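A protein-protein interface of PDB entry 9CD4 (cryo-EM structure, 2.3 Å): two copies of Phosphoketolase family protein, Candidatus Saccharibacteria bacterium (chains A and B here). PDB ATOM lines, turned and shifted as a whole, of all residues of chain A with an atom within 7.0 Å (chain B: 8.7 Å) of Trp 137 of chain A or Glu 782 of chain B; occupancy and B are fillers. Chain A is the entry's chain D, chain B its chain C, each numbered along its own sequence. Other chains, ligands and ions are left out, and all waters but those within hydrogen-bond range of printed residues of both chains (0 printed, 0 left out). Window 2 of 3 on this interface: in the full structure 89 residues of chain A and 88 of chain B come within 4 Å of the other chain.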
ATOM      1  N   LEU A  39      28.575  18.842  33.522  1.00  0.00           N
ATOM      2  CA  LEU A  39      27.665  19.935  33.848  1.00  0.00           C
ATOM      3  C   LEU A  39      26.498  20.046  32.875  1.00  0.00           C
ATOM      4  O   LEU A  39      26.631  19.798  31.674  1.00  0.00           O
ATOM      5  CB  LEU A  39      28.417  21.263  33.891  1.00  0.00           C
ATOM      6  CG  LEU A  39      29.401  21.474  35.041  1.00  0.00           C
ATOM      7  CD1 LEU A  39      29.602  22.959  35.256  1.00  0.00           C
ATOM      8  CD2 LEU A  39      28.924  20.803  36.319  1.00  0.00           C
ATOM      9  N   GLN A  40      25.342  20.427  33.423  1.00  0.00           N
ATOM     10  CA  GLN A  40      24.156  20.788  32.663  1.00  0.00           C
ATOM     11  C   GLN A  40      23.848  22.277  32.739  1.00  0.00           C
ATOM     12  O   GLN A  40      23.210  22.813  31.827  1.00  0.00           O
ATOM     13  CB  GLN A  40      22.946  19.987  33.174  1.00  0.00           C
ATOM     14  CG  GLN A  40      21.666  20.122  32.365  1.00  0.00           C
ATOM     15  CD  GLN A  40      20.457  19.583  33.106  1.00  0.00           C
ATOM     16  OE1 GLN A  40      20.570  19.091  34.227  1.00  0.00           O
ATOM     17  NE2 GLN A  40      19.290  19.677  32.481  1.00  0.00           N
ATOM     18  N   LYS A  55      24.078  16.623  34.942  1.00  0.00           N
ATOM     19  CA  LYS A  55      23.297  15.912  33.941  1.00  0.00           C
ATOM     20  C   LYS A  55      22.610  14.704  34.573  1.00  0.00           C
ATOM     21  O   LYS A  55      23.189  14.049  35.448  1.00  0.00           O
ATOM     22  CB  LYS A  55      24.188  15.462  32.783  1.00  0.00           C
ATOM     23  CG  LYS A  55      24.532  16.563  31.793  1.00  0.00           C
ATOM     24  CD  LYS A  55      25.017  15.985  30.474  1.00  0.00           C
ATOM     25  CE  LYS A  55      25.763  17.025  29.654  1.00  0.00           C
ATOM     26  NZ  LYS A  55      27.235  16.948  29.860  1.00  0.00           N
ATOM     27  N   PRO A  56      21.369  14.398  34.177  1.00  0.00           N
ATOM     28  CA  PRO A  56      20.676  13.234  34.756  1.00  0.00           C
ATOM     29  C   PRO A  56      21.376  11.912  34.495  1.00  0.00           C
ATOM     30  O   PRO A  56      21.343  11.023  35.355  1.00  0.00           O
ATOM     31  CB  PRO A  56      19.294  13.279  34.089  1.00  0.00           C
ATOM     32  CG  PRO A  56      19.148  14.675  33.580  1.00  0.00           C
ATOM     33  CD  PRO A  56      20.522  15.131  33.223  1.00  0.00           C
ATOM     34  N   ARG A  57      22.012  11.753  33.336  1.00  0.00           N
ATOM     35  CA  ARG A  57      22.774  10.556  33.008  1.00  0.00           C
ATOM     36  C   ARG A  57      24.202  10.968  32.692  1.00  0.00           C
ATOM     37  O   ARG A  57      24.430  11.789  31.798  1.00  0.00           O
ATOM     38  CB  ARG A  57      22.150   9.808  31.828  1.00  0.00           C
ATOM     39  CG  ARG A  57      20.776   9.231  32.120  1.00  0.00           C
ATOM     40  CD  ARG A  57      20.331   8.278  31.023  1.00  0.00           C
ATOM     41  NE  ARG A  57      19.705   8.975  29.907  1.00  0.00           N
ATOM     42  CZ  ARG A  57      20.013   8.776  28.633  1.00  0.00           C
ATOM     43  NH1 ARG A  57      20.944   7.908  28.273  1.00  0.00           N
ATOM     44  NH2 ARG A  57      19.370   9.466  27.695  1.00  0.00           N
ATOM     45  N   LEU A  59      27.304  10.118  31.028  1.00  0.00           N
ATOM     46  CA  LEU A  59      27.898   9.289  29.992  1.00  0.00           C
ATOM     47  C   LEU A  59      29.206   9.908  29.519  1.00  0.00           C
ATOM     48  O   LEU A  59      29.392  11.127  29.577  1.00  0.00           O
ATOM     49  CB  LEU A  59      26.942   9.120  28.808  1.00  0.00           C
ATOM     50  CG  LEU A  59      25.474   8.875  29.160  1.00  0.00           C
ATOM     51  CD1 LEU A  59      24.573   9.227  27.988  1.00  0.00           C
ATOM     52  CD2 LEU A  59      25.261   7.432  29.584  1.00  0.00           C
ATOM     53  N   SER A 132      28.991  22.336  25.841  1.00  0.00           N
ATOM     54  CA  SER A 132      28.939  21.565  27.079  1.00  0.00           C
ATOM     55  C   SER A 132      27.580  20.902  27.278  1.00  0.00           C
ATOM     56  O   SER A 132      27.511  19.749  27.717  1.00  0.00           O
ATOM     57  CB  SER A 132      29.271  22.463  28.269  1.00  0.00           C
ATOM     58  OG  SER A 132      30.641  22.823  28.271  1.00  0.00           O
ATOM     59  N   LYS A 133      26.497  21.613  26.967  1.00  0.00           N
ATOM     60  CA  LYS A 133      25.160  21.077  27.202  1.00  0.00           C
ATOM     61  C   LYS A 133      24.837  19.931  26.250  1.00  0.00           C
ATOM     62  O   LYS A 133      24.222  18.936  26.652  1.00  0.00           O
ATOM     63  CB  LYS A 133      24.126  22.197  27.071  1.00  0.00           C
ATOM     64  CG  LYS A 133      22.681  21.733  27.002  1.00  0.00           C
ATOM     65  CD  LYS A 133      22.194  21.236  28.350  1.00  0.00           C
ATOM     66  CE  LYS A 133      20.690  21.036  28.349  1.00  0.00           C
ATOM     67  NZ  LYS A 133      19.956  22.329  28.276  1.00  0.00           N
ATOM     68  N   ASN A 134      25.259  20.039  24.993  1.00  0.00           N
ATOM     69  CA  ASN A 134      24.821  19.122  23.950  1.00  0.00           C
ATOM     70  C   ASN A 134      25.710  17.895  23.798  1.00  0.00           C
ATOM     71  O   ASN A 134      25.471  17.091  22.891  1.00  0.00           O
ATOM     72  CB  ASN A 134      24.729  19.859  22.610  1.00  0.00           C
ATOM     73  CG  ASN A 134      23.451  20.660  22.474  1.00  0.00           C
ATOM     74  OD1 ASN A 134      22.436  20.155  21.996  1.00  0.00           O
ATOM     75  ND2 ASN A 134      23.494  21.917  22.898  1.00  0.00           N
ATOM     76  N   PHE A 135      26.722  17.724  24.645  1.00  0.00           N
ATOM     77  CA  PHE A 135      27.534  16.516  24.583  1.00  0.00           C
ATOM     78  C   PHE A 135      26.748  15.334  25.137  1.00  0.00           C
ATOM     79  O   PHE A 135      26.231  15.389  26.257  1.00  0.00           O
ATOM     80  CB  PHE A 135      28.833  16.696  25.363  1.00  0.00           C
ATOM     81  CG  PHE A 135      29.630  15.430  25.503  1.00  0.00           C
ATOM     82  CD1 PHE A 135      30.263  14.871  24.407  1.00  0.00           C
ATOM     83  CD2 PHE A 135      29.737  14.793  26.729  1.00  0.00           C
ATOM     84  CE1 PHE A 135      30.995  13.706  24.530  1.00  0.00           C
ATOM     85  CE2 PHE A 135      30.467  13.627  26.858  1.00  0.00           C
ATOM     86  CZ  PHE A 135      31.095  13.082  25.758  1.00  0.00           C
ATOM     87  N   SER A 136      26.644  14.272  24.335  1.00  0.00           N
ATOM     88  CA  SER A 136      25.916  13.041  24.633  1.00  0.00           C
ATOM     89  C   SER A 136      24.424  13.265  24.865  1.00  0.00           C
ATOM     90  O   SER A 136      23.730  12.351  25.324  1.00  0.00           O
ATOM     91  CB  SER A 136      26.524  12.296  25.831  1.00  0.00           C
ATOM     92  OG  SER A 136      27.910  12.069  25.639  1.00  0.00           O
ATOM     93  N   TRP A 137      23.912  14.453  24.563  1.00  0.00           N
ATOM     94  CA  TRP A 137      22.493  14.744  24.646  1.00  0.00           C
ATOM     95  C   TRP A 137      21.767  14.143  23.444  1.00  0.00           C
ATOM     96  O   TRP A 137      22.342  14.028  22.360  1.00  0.00           O
ATOM     97  CB  TRP A 137      22.265  16.252  24.689  1.00  0.00           C
ATOM     98  CG  TRP A 137      21.008  16.677  25.388  1.00  0.00           C
ATOM     99  CD1 TRP A 137      19.780  16.868  24.824  1.00  0.00           C
ATOM    100  CD2 TRP A 137      20.859  16.977  26.781  1.00  0.00           C
ATOM    101  NE1 TRP A 137      18.875  17.261  25.779  1.00  0.00           N
ATOM    102  CE2 TRP A 137      19.513  17.336  26.989  1.00  0.00           C
ATOM    103  CE3 TRP A 137      21.732  16.974  27.873  1.00  0.00           C
ATOM    104  CZ2 TRP A 137      19.019  17.690  28.243  1.00  0.00           C
ATOM    105  CZ3 TRP A 137      21.240  17.325  29.117  1.00  0.00           C
ATOM    106  CH2 TRP A 137      19.896  17.676  29.291  1.00  0.00           C
ATOM    107  N   PRO A 138      20.507  13.730  23.617  1.00  0.00           N
ATOM    108  CA  PRO A 138      19.715  13.300  22.457  1.00  0.00           C
ATOM    109  C   PRO A 138      19.490  14.439  21.474  1.00  0.00           C
ATOM    110  O   PRO A 138      18.783  15.403  21.777  1.00  0.00           O
ATOM    111  CB  PRO A 138      18.399  12.825  23.084  1.00  0.00           C
ATOM    112  CG  PRO A 138      18.762  12.449  24.476  1.00  0.00           C
ATOM    113  CD  PRO A 138      19.849  13.396  24.891  1.00  0.00           C
ATOM    114  N   GLY A 139      20.090  14.330  20.291  1.00  0.00           N
ATOM    115  CA  GLY A 139      20.039  15.381  19.299  1.00  0.00           C
ATOM    116  C   GLY A 139      21.253  16.281  19.255  1.00  0.00           C
ATOM    117  O   GLY A 139      21.316  17.163  18.391  1.00  0.00           O
ATOM    118  N   GLY A 140      22.212  16.092  20.151  1.00  0.00           N
ATOM    119  CA  GLY A 140      23.424  16.881  20.201  1.00  0.00           C
ATOM    120  C   GLY A 140      24.616  16.147  19.623  1.00  0.00           C
ATOM    121  O   GLY A 140      24.483  15.300  18.731  1.00  0.00           O
ATOM    122  N   PHE A 141      25.797  16.479  20.131  1.00  0.00           N
ATOM    123  CA  PHE A 141      27.011  15.819  19.677  1.00  0.00           C
ATOM    124  C   PHE A 141      27.048  14.377  20.178  1.00  0.00           C
ATOM    125  O   PHE A 141      26.673  14.107  21.323  1.00  0.00           O
ATOM    126  CB  PHE A 141      28.249  16.571  20.165  1.00  0.00           C
ATOM    127  CG  PHE A 141      28.313  17.999  19.707  1.00  0.00           C
ATOM    128  CD1 PHE A 141      28.664  18.307  18.402  1.00  0.00           C
ATOM    129  CD2 PHE A 141      28.024  19.035  20.580  1.00  0.00           C
ATOM    130  CE1 PHE A 141      28.724  19.621  17.978  1.00  0.00           C
ATOM    131  CE2 PHE A 141      28.083  20.350  20.161  1.00  0.00           C
ATOM    132  CZ  PHE A 141      28.434  20.643  18.859  1.00  0.00           C
ATOM    133  N   PRO A 142      27.485  13.433  19.349  1.00  0.00           N
ATOM    134  CA  PRO A 142      27.610  12.044  19.806  1.00  0.00           C
ATOM    135  C   PRO A 142      28.763  11.889  20.787  1.00  0.00           C
ATOM    136  O   PRO A 142      29.632  12.751  20.922  1.00  0.00           O
ATOM    137  CB  PRO A 142      27.866  11.257  18.515  1.00  0.00           C
ATOM    138  CG  PRO A 142      27.491  12.188  17.399  1.00  0.00           C
ATOM    139  CD  PRO A 142      27.766  13.564  17.911  1.00  0.00           C
ATOM    140  N   SER A 143      28.753  10.756  21.489  1.00  0.00           N
ATOM    141  CA  SER A 143      29.784  10.466  22.476  1.00  0.00           C
ATOM    142  C   SER A 143      31.087   9.979  21.856  1.00  0.00           C
ATOM    143  O   SER A 143      32.104   9.935  22.555  1.00  0.00           O
ATOM    144  CB  SER A 143      29.273   9.424  23.474  1.00  0.00           C
ATOM    145  OG  SER A 143      28.387   8.512  22.848  1.00  0.00           O
ATOM    146  N   ASP B 530      24.858   2.686  25.835  1.00  0.00           N
ATOM    147  CA  ASP B 530      24.620   4.016  26.381  1.00  0.00           C
ATOM    148  C   ASP B 530      25.844   4.918  26.293  1.00  0.00           C
ATOM    149  O   ASP B 530      25.711   6.111  26.000  1.00  0.00           O
ATOM    150  CB  ASP B 530      24.160   3.905  27.837  1.00  0.00           C
ATOM    151  CG  ASP B 530      22.808   3.236  27.969  1.00  0.00           C
ATOM    152  OD1 ASP B 530      21.977   3.386  27.049  1.00  0.00           O
ATOM    153  OD2 ASP B 530      22.575   2.555  28.990  1.00  0.00           O
ATOM    154  N   SER B 729      21.893   6.435  17.180  1.00  0.00           N
ATOM    155  CA  SER B 729      23.028   7.172  17.723  1.00  0.00           C
ATOM    156  C   SER B 729      22.913   7.161  19.244  1.00  0.00           C
ATOM    157  O   SER B 729      22.101   6.424  19.815  1.00  0.00           O
ATOM    158  CB  SER B 729      23.080   8.597  17.162  1.00  0.00           C
ATOM    159  OG  SER B 729      21.859   9.277  17.388  1.00  0.00           O
ATOM    160  N   THR B 730      23.728   7.981  19.902  1.00  0.00           N
ATOM    161  CA  THR B 730      23.698   8.102  21.359  1.00  0.00           C
ATOM    162  C   THR B 730      22.425   8.830  21.769  1.00  0.00           C
ATOM    163  O   THR B 730      22.323  10.051  21.634  1.00  0.00           O
ATOM    164  CB  THR B 730      24.934   8.841  21.858  1.00  0.00           C
ATOM    165  OG1 THR B 730      26.101   8.321  21.205  1.00  0.00           O
ATOM    166  CG2 THR B 730      25.084   8.673  23.360  1.00  0.00           C
ATOM    167  N   THR B 731      21.450   8.084  22.277  1.00  0.00           N
ATOM    168  CA  THR B 731      20.159   8.646  22.657  1.00  0.00           C
ATOM    169  C   THR B 731      19.506   7.719  23.677  1.00  0.00           C
ATOM    170  O   THR B 731      20.131   6.775  24.173  1.00  0.00           O
ATOM    171  CB  THR B 731      19.271   8.851  21.425  1.00  0.00           C
ATOM    172  OG1 THR B 731      18.023   9.431  21.824  1.00  0.00           O
ATOM    173  CG2 THR B 731      19.012   7.523  20.727  1.00  0.00           C
ATOM    174  N   THR B 732      18.242   7.993  23.993  1.00  0.00           N
ATOM    175  CA  THR B 732      17.479   7.188  24.932  1.00  0.00           C
ATOM    176  C   THR B 732      17.093   5.851  24.303  1.00  0.00           C
ATOM    177  O   THR B 732      17.026   5.730  23.077  1.00  0.00           O
ATOM    178  CB  THR B 732      16.229   7.943  25.373  1.00  0.00           C
ATOM    179  OG1 THR B 732      15.271   7.952  24.307  1.00  0.00           O
ATOM    180  CG2 THR B 732      16.576   9.373  25.748  1.00  0.00           C
ATOM    181  N   ASP B 735      14.013   6.140  22.024  1.00  0.00           N
ATOM    182  CA  ASP B 735      14.376   6.738  20.743  1.00  0.00           C
ATOM    183  C   ASP B 735      15.115   5.739  19.863  1.00  0.00           C
ATOM    184  O   ASP B 735      14.912   5.704  18.644  1.00  0.00           O
ATOM    185  CB  ASP B 735      15.227   7.988  20.971  1.00  0.00           C
ATOM    186  CG  ASP B 735      15.349   8.848  19.727  1.00  0.00           C
ATOM    187  OD1 ASP B 735      14.307   9.188  19.130  1.00  0.00           O
ATOM    188  OD2 ASP B 735      16.488   9.188  19.347  1.00  0.00           O
ATOM    189  N   ARG B 739      13.612   4.728  16.234  1.00  0.00           N
ATOM    190  CA  ARG B 739      14.333   5.075  15.013  1.00  0.00           C
ATOM    191  C   ARG B 739      14.302   3.943  13.993  1.00  0.00           C
ATOM    192  O   ARG B 739      14.296   4.199  12.785  1.00  0.00           O
ATOM    193  CB  ARG B 739      15.779   5.446  15.339  1.00  0.00           C
ATOM    194  CG  ARG B 739      15.963   6.878  15.802  1.00  0.00           C
ATOM    195  CD  ARG B 739      17.432   7.256  15.849  1.00  0.00           C
ATOM    196  NE  ARG B 739      17.668   8.411  16.706  1.00  0.00           N
ATOM    197  CZ  ARG B 739      18.813   9.076  16.769  1.00  0.00           C
ATOM    198  NH1 ARG B 739      19.857   8.725  16.036  1.00  0.00           N
ATOM    199  NH2 ARG B 739      18.915  10.116  17.591  1.00  0.00           N
ATOM    200  N   ASP B 774       5.356  10.912  19.296  1.00  0.00           N
ATOM    201  CA  ASP B 774       5.966  12.227  19.129  1.00  0.00           C
ATOM    202  C   ASP B 774       6.180  12.915  20.471  1.00  0.00           C
ATOM    203  O   ASP B 774       7.226  13.532  20.699  1.00  0.00           O
ATOM    204  CB  ASP B 774       5.096  13.094  18.218  1.00  0.00           C
ATOM    205  CG  ASP B 774       5.446  12.936  16.753  1.00  0.00           C
ATOM    206  OD1 ASP B 774       6.603  12.577  16.451  1.00  0.00           O
ATOM    207  OD2 ASP B 774       4.561  13.171  15.903  1.00  0.00           O
ATOM    208  N   ASP B 775       5.196  12.822  21.369  1.00  0.00           N
ATOM    209  CA  ASP B 775       5.335  13.418  22.693  1.00  0.00           C
ATOM    210  C   ASP B 775       6.445  12.744  23.490  1.00  0.00           C
ATOM    211  O   ASP B 775       7.214  13.415  24.190  1.00  0.00           O
ATOM    212  CB  ASP B 775       4.008  13.335  23.449  1.00  0.00           C
ATOM    213  CG  ASP B 775       2.962  14.278  22.892  1.00  0.00           C
ATOM    214  OD1 ASP B 775       3.307  15.111  22.028  1.00  0.00           O
ATOM    215  OD2 ASP B 775       1.792  14.189  23.321  1.00  0.00           O
ATOM    216  N   ALA B 776       6.541  11.413  23.398  1.00  0.00           N
ATOM    217  CA  ALA B 776       7.610  10.699  24.090  1.00  0.00           C
ATOM    218  C   ALA B 776       8.981  11.100  23.558  1.00  0.00           C
ATOM    219  O   ALA B 776       9.922  11.307  24.337  1.00  0.00           O
ATOM    220  CB  ALA B 776       7.401   9.191  23.960  1.00  0.00           C
ATOM    221  N   LEU B 777       9.112  11.224  22.235  1.00  0.00           N
ATOM    222  CA  LEU B 777      10.385  11.638  21.651  1.00  0.00           C
ATOM    223  C   LEU B 777      10.728  13.074  22.028  1.00  0.00           C
ATOM    224  O   LEU B 777      11.897  13.394  22.266  1.00  0.00           O
ATOM    225  CB  LEU B 777      10.350  11.472  20.133  1.00  0.00           C
ATOM    226  CG  LEU B 777      10.241  10.036  19.614  1.00  0.00           C
ATOM    227  CD1 LEU B 777      10.377   9.992  18.099  1.00  0.00           C
ATOM    228  CD2 LEU B 777      11.263   9.133  20.283  1.00  0.00           C
ATOM    229  N   ARG B 778       9.722  13.953  22.086  1.00  0.00           N
ATOM    230  CA  ARG B 778       9.956  15.329  22.515  1.00  0.00           C
ATOM    231  C   ARG B 778      10.425  15.387  23.963  1.00  0.00           C
ATOM    232  O   ARG B 778      11.338  16.152  24.298  1.00  0.00           O
ATOM    233  CB  ARG B 778       8.685  16.157  22.334  1.00  0.00           C
ATOM    234  CG  ARG B 778       8.673  17.016  21.086  1.00  0.00           C
ATOM    235  CD  ARG B 778       7.602  18.090  21.171  1.00  0.00           C
ATOM    236  NE  ARG B 778       6.262  17.537  21.021  1.00  0.00           N
ATOM    237  CZ  ARG B 778       5.692  17.258  19.856  1.00  0.00           C
ATOM    238  NH1 ARG B 778       6.320  17.467  18.710  1.00  0.00           N
ATOM    239  NH2 ARG B 778       4.461  16.756  19.841  1.00  0.00           N
ATOM    240  N   PHE B 779       9.803  14.590  24.838  1.00  0.00           N
ATOM    241  CA  PHE B 779      10.230  14.539  26.233  1.00  0.00           C
ATOM    242  C   PHE B 779      11.657  14.022  26.352  1.00  0.00           C
ATOM    243  O   PHE B 779      12.458  14.560  27.126  1.00  0.00           O
ATOM    244  CB  PHE B 779       9.269  13.664  27.042  1.00  0.00           C
ATOM    245  CG  PHE B 779       9.261  13.966  28.517  1.00  0.00           C
ATOM    246  CD1 PHE B 779      10.291  13.531  29.338  1.00  0.00           C
ATOM    247  CD2 PHE B 779       8.220  14.684  29.082  1.00  0.00           C
ATOM    248  CE1 PHE B 779      10.284  13.808  30.692  1.00  0.00           C
ATOM    249  CE2 PHE B 779       8.208  14.964  30.435  1.00  0.00           C
ATOM    250  CZ  PHE B 779       9.241  14.525  31.241  1.00  0.00           C
ATOM    251  N   ALA B 780      11.993  12.977  25.587  1.00  0.00           N
ATOM    252  CA  ALA B 780      13.350  12.441  25.615  1.00  0.00           C
ATOM    253  C   ALA B 780      14.362  13.462  25.110  1.00  0.00           C
ATOM    254  O   ALA B 780      15.469  13.570  25.651  1.00  0.00           O
ATOM    255  CB  ALA B 780      13.423  11.158  24.786  1.00  0.00           C
ATOM    256  N   GLN B 781      14.004  14.213  24.065  1.00  0.00           N
ATOM    257  CA  GLN B 781      14.897  15.240  23.539  1.00  0.00           C
ATOM    258  C   GLN B 781      15.105  16.370  24.540  1.00  0.00           C
ATOM    259  O   GLN B 781      16.231  16.848  24.718  1.00  0.00           O
ATOM    260  CB  GLN B 781      14.340  15.791  22.227  1.00  0.00           C
ATOM    261  CG  GLN B 781      15.127  15.392  20.992  1.00  0.00           C
ATOM    262  CD  GLN B 781      14.266  15.345  19.746  1.00  0.00           C
ATOM    263  OE1 GLN B 781      13.177  15.917  19.709  1.00  0.00           O
ATOM    264  NE2 GLN B 781      14.751  14.661  18.717  1.00  0.00           N
ATOM    265  N   GLU B 782      14.033  16.812  25.199  1.00  0.00           N
ATOM    266  CA  GLU B 782      14.134  17.973  26.077  1.00  0.00           C
ATOM    267  C   GLU B 782      14.791  17.639  27.412  1.00  0.00           C
ATOM    268  O   GLU B 782      15.562  18.448  27.940  1.00  0.00           O
ATOM    269  CB  GLU B 782      12.750  18.578  26.306  1.00  0.00           C
ATOM    270  CG  GLU B 782      12.170  19.272  25.087  1.00  0.00           C
ATOM    271  CD  GLU B 782      10.661  19.397  25.151  1.00  0.00           C
ATOM    272  OE1 GLU B 782      10.074  18.999  26.179  1.00  0.00           O
ATOM    273  OE2 GLU B 782      10.063  19.895  24.173  1.00  0.00           O
ATOM    274  N   ASN B 783      14.512  16.461  27.972  1.00  0.00           N
ATOM    275  CA  ASN B 783      14.907  16.160  29.341  1.00  0.00           C
ATOM    276  C   ASN B 783      16.076  15.191  29.461  1.00  0.00           C
ATOM    277  O   ASN B 783      16.558  14.979  30.579  1.00  0.00           O
ATOM    278  CB  ASN B 783      13.711  15.598  30.123  1.00  0.00           C
ATOM    279  CG  ASN B 783      12.585  16.601  30.259  1.00  0.00           C
ATOM    280  OD1 ASN B 783      12.572  17.413  31.183  1.00  0.00           O
ATOM    281  ND2 ASN B 783      11.635  16.553  29.335  1.00  0.00           N
ATOM    282  N   SER B 784      16.523  14.587  28.359  1.00  0.00           N
ATOM    283  CA  SER B 784      17.596  13.593  28.307  1.00  0.00           C
ATOM    284  C   SER B 784      17.293  12.341  29.123  1.00  0.00           C
ATOM    285  O   SER B 784      18.200  11.540  29.382  1.00  0.00           O
ATOM    286  CB  SER B 784      18.946  14.180  28.744  1.00  0.00           C
ATOM    287  OG  SER B 784      19.951  13.183  28.780  1.00  0.00           O
ATOM    288  N   VAL B 785      16.040  12.150  29.542  1.00  0.00           N
ATOM    289  CA  VAL B 785      15.594  10.936  30.208  1.00  0.00           C
ATOM    290  C   VAL B 785      14.258  10.541  29.599  1.00  0.00           C
ATOM    291  O   VAL B 785      13.552  11.361  29.009  1.00  0.00           O
ATOM    292  CB  VAL B 785      15.452  11.099  31.738  1.00  0.00           C
ATOM    293  CG1 VAL B 785      16.818  11.167  32.399  1.00  0.00           C
ATOM    294  CG2 VAL B 785      14.629  12.334  32.068  1.00  0.00           C
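The side-chain hydroxyl (OG) of Ser 143 of chain A sits at hydrogen-bond distance from the side-chain hydroxyl (OG1) of Thr 730 of chain B (2.8 Å).
The backbone carbonyl oxygen of Gln 781 of chain B is in hydrogen-bond range of the indole nitrogen of Trp 137 of chain A, 2.9 Å away.
The guanidinium group (NH2) of Arg 57 of chain A sits at hydrogen-bond distance from the backbone carbonyl oxygen (O) of Ser 784 of chain B.
The side-chain hydroxyl (OG1) of Thr 731 of chain B is in hydrogen-bond range of the side-chain carboxylate (OD2) of Asp 735 of chain B.
OG1 of Thr 732 of chain B is in hydrogen-bond range of N of Asp 735 of chain B (3.2 Å).
O of Phe 779 of chain B is in hydrogen-bond range of ND2 of Asn 783 of chain B, 3.1 Å away.
Asn 783 of chain B touches Pro 56 of chain A.
Arg 57 of chain A touches Thr 732 of chain B (NH2 to CG2, 3.4 Å).
CD2 of Leu 59 of chain A touches O of Asp 530 of chain B (3.8 Å).
O of Glu 782 of chain B touches CZ2 of Trp 137 of chain A, 3.6 Å away.
Trp 137 of chain A touches Ser 784 of chain B (CZ2 to CB, 3.5 Å).
OG1 of Thr 731 of chain B touches CB of Pro 138 of chain A, 3.6 Å away.
Pro 138 of chain A touches Thr 732 of chain B.
Pro 138 of chain A touches Ala 780 of chain B.
O of Pro 138 of chain A touches CG of Gln 781 of chain B, at 3.7 Å.
OG of Ser 784 of chain B touches CD of Pro 138 of chain A, at 3.9 Å.
Lys 133 of chain A touches none of the printed residues of chain B.
Ser 136 of chain A touches none of the printed residues of chain B.
Of the printed residues of chain B, Trp 137 of chain A touches Gln 781 (2.9 Å), Glu 782 (3.6 Å) and Ser 784 (3.5 Å).
Gly 140 of chain A touches none of the printed residues of chain B.
Printed residues of chain A within 4 Å of Asp 530 of chain B: Leu 59 (3.8 Å).
Printed residues of chain A within 4 Å of Ala 780 of chain B: Pro 138.
Glu 782 of chain B touches just one residue of chain A: Trp 137 (3.6 Å).
The nearest printed residue of chain A that does not touch Thr 730 of chain B is Trp 137 of chain A (4.04 Å).
Hydrophobic or aromatic side chains of chain B that line the printed part of chain A: Val 785.
Of the 18 printed residues of chain A, 6 touch a printed residue of chain B.
Among the printed residues, 14 pairs touch across the chains.
Among the printed residues, no Asp or Glu carboxylate lies within 4 Å of a Lys or Arg side-chain nitrogen of the other chain.
No position is printed for both chains.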
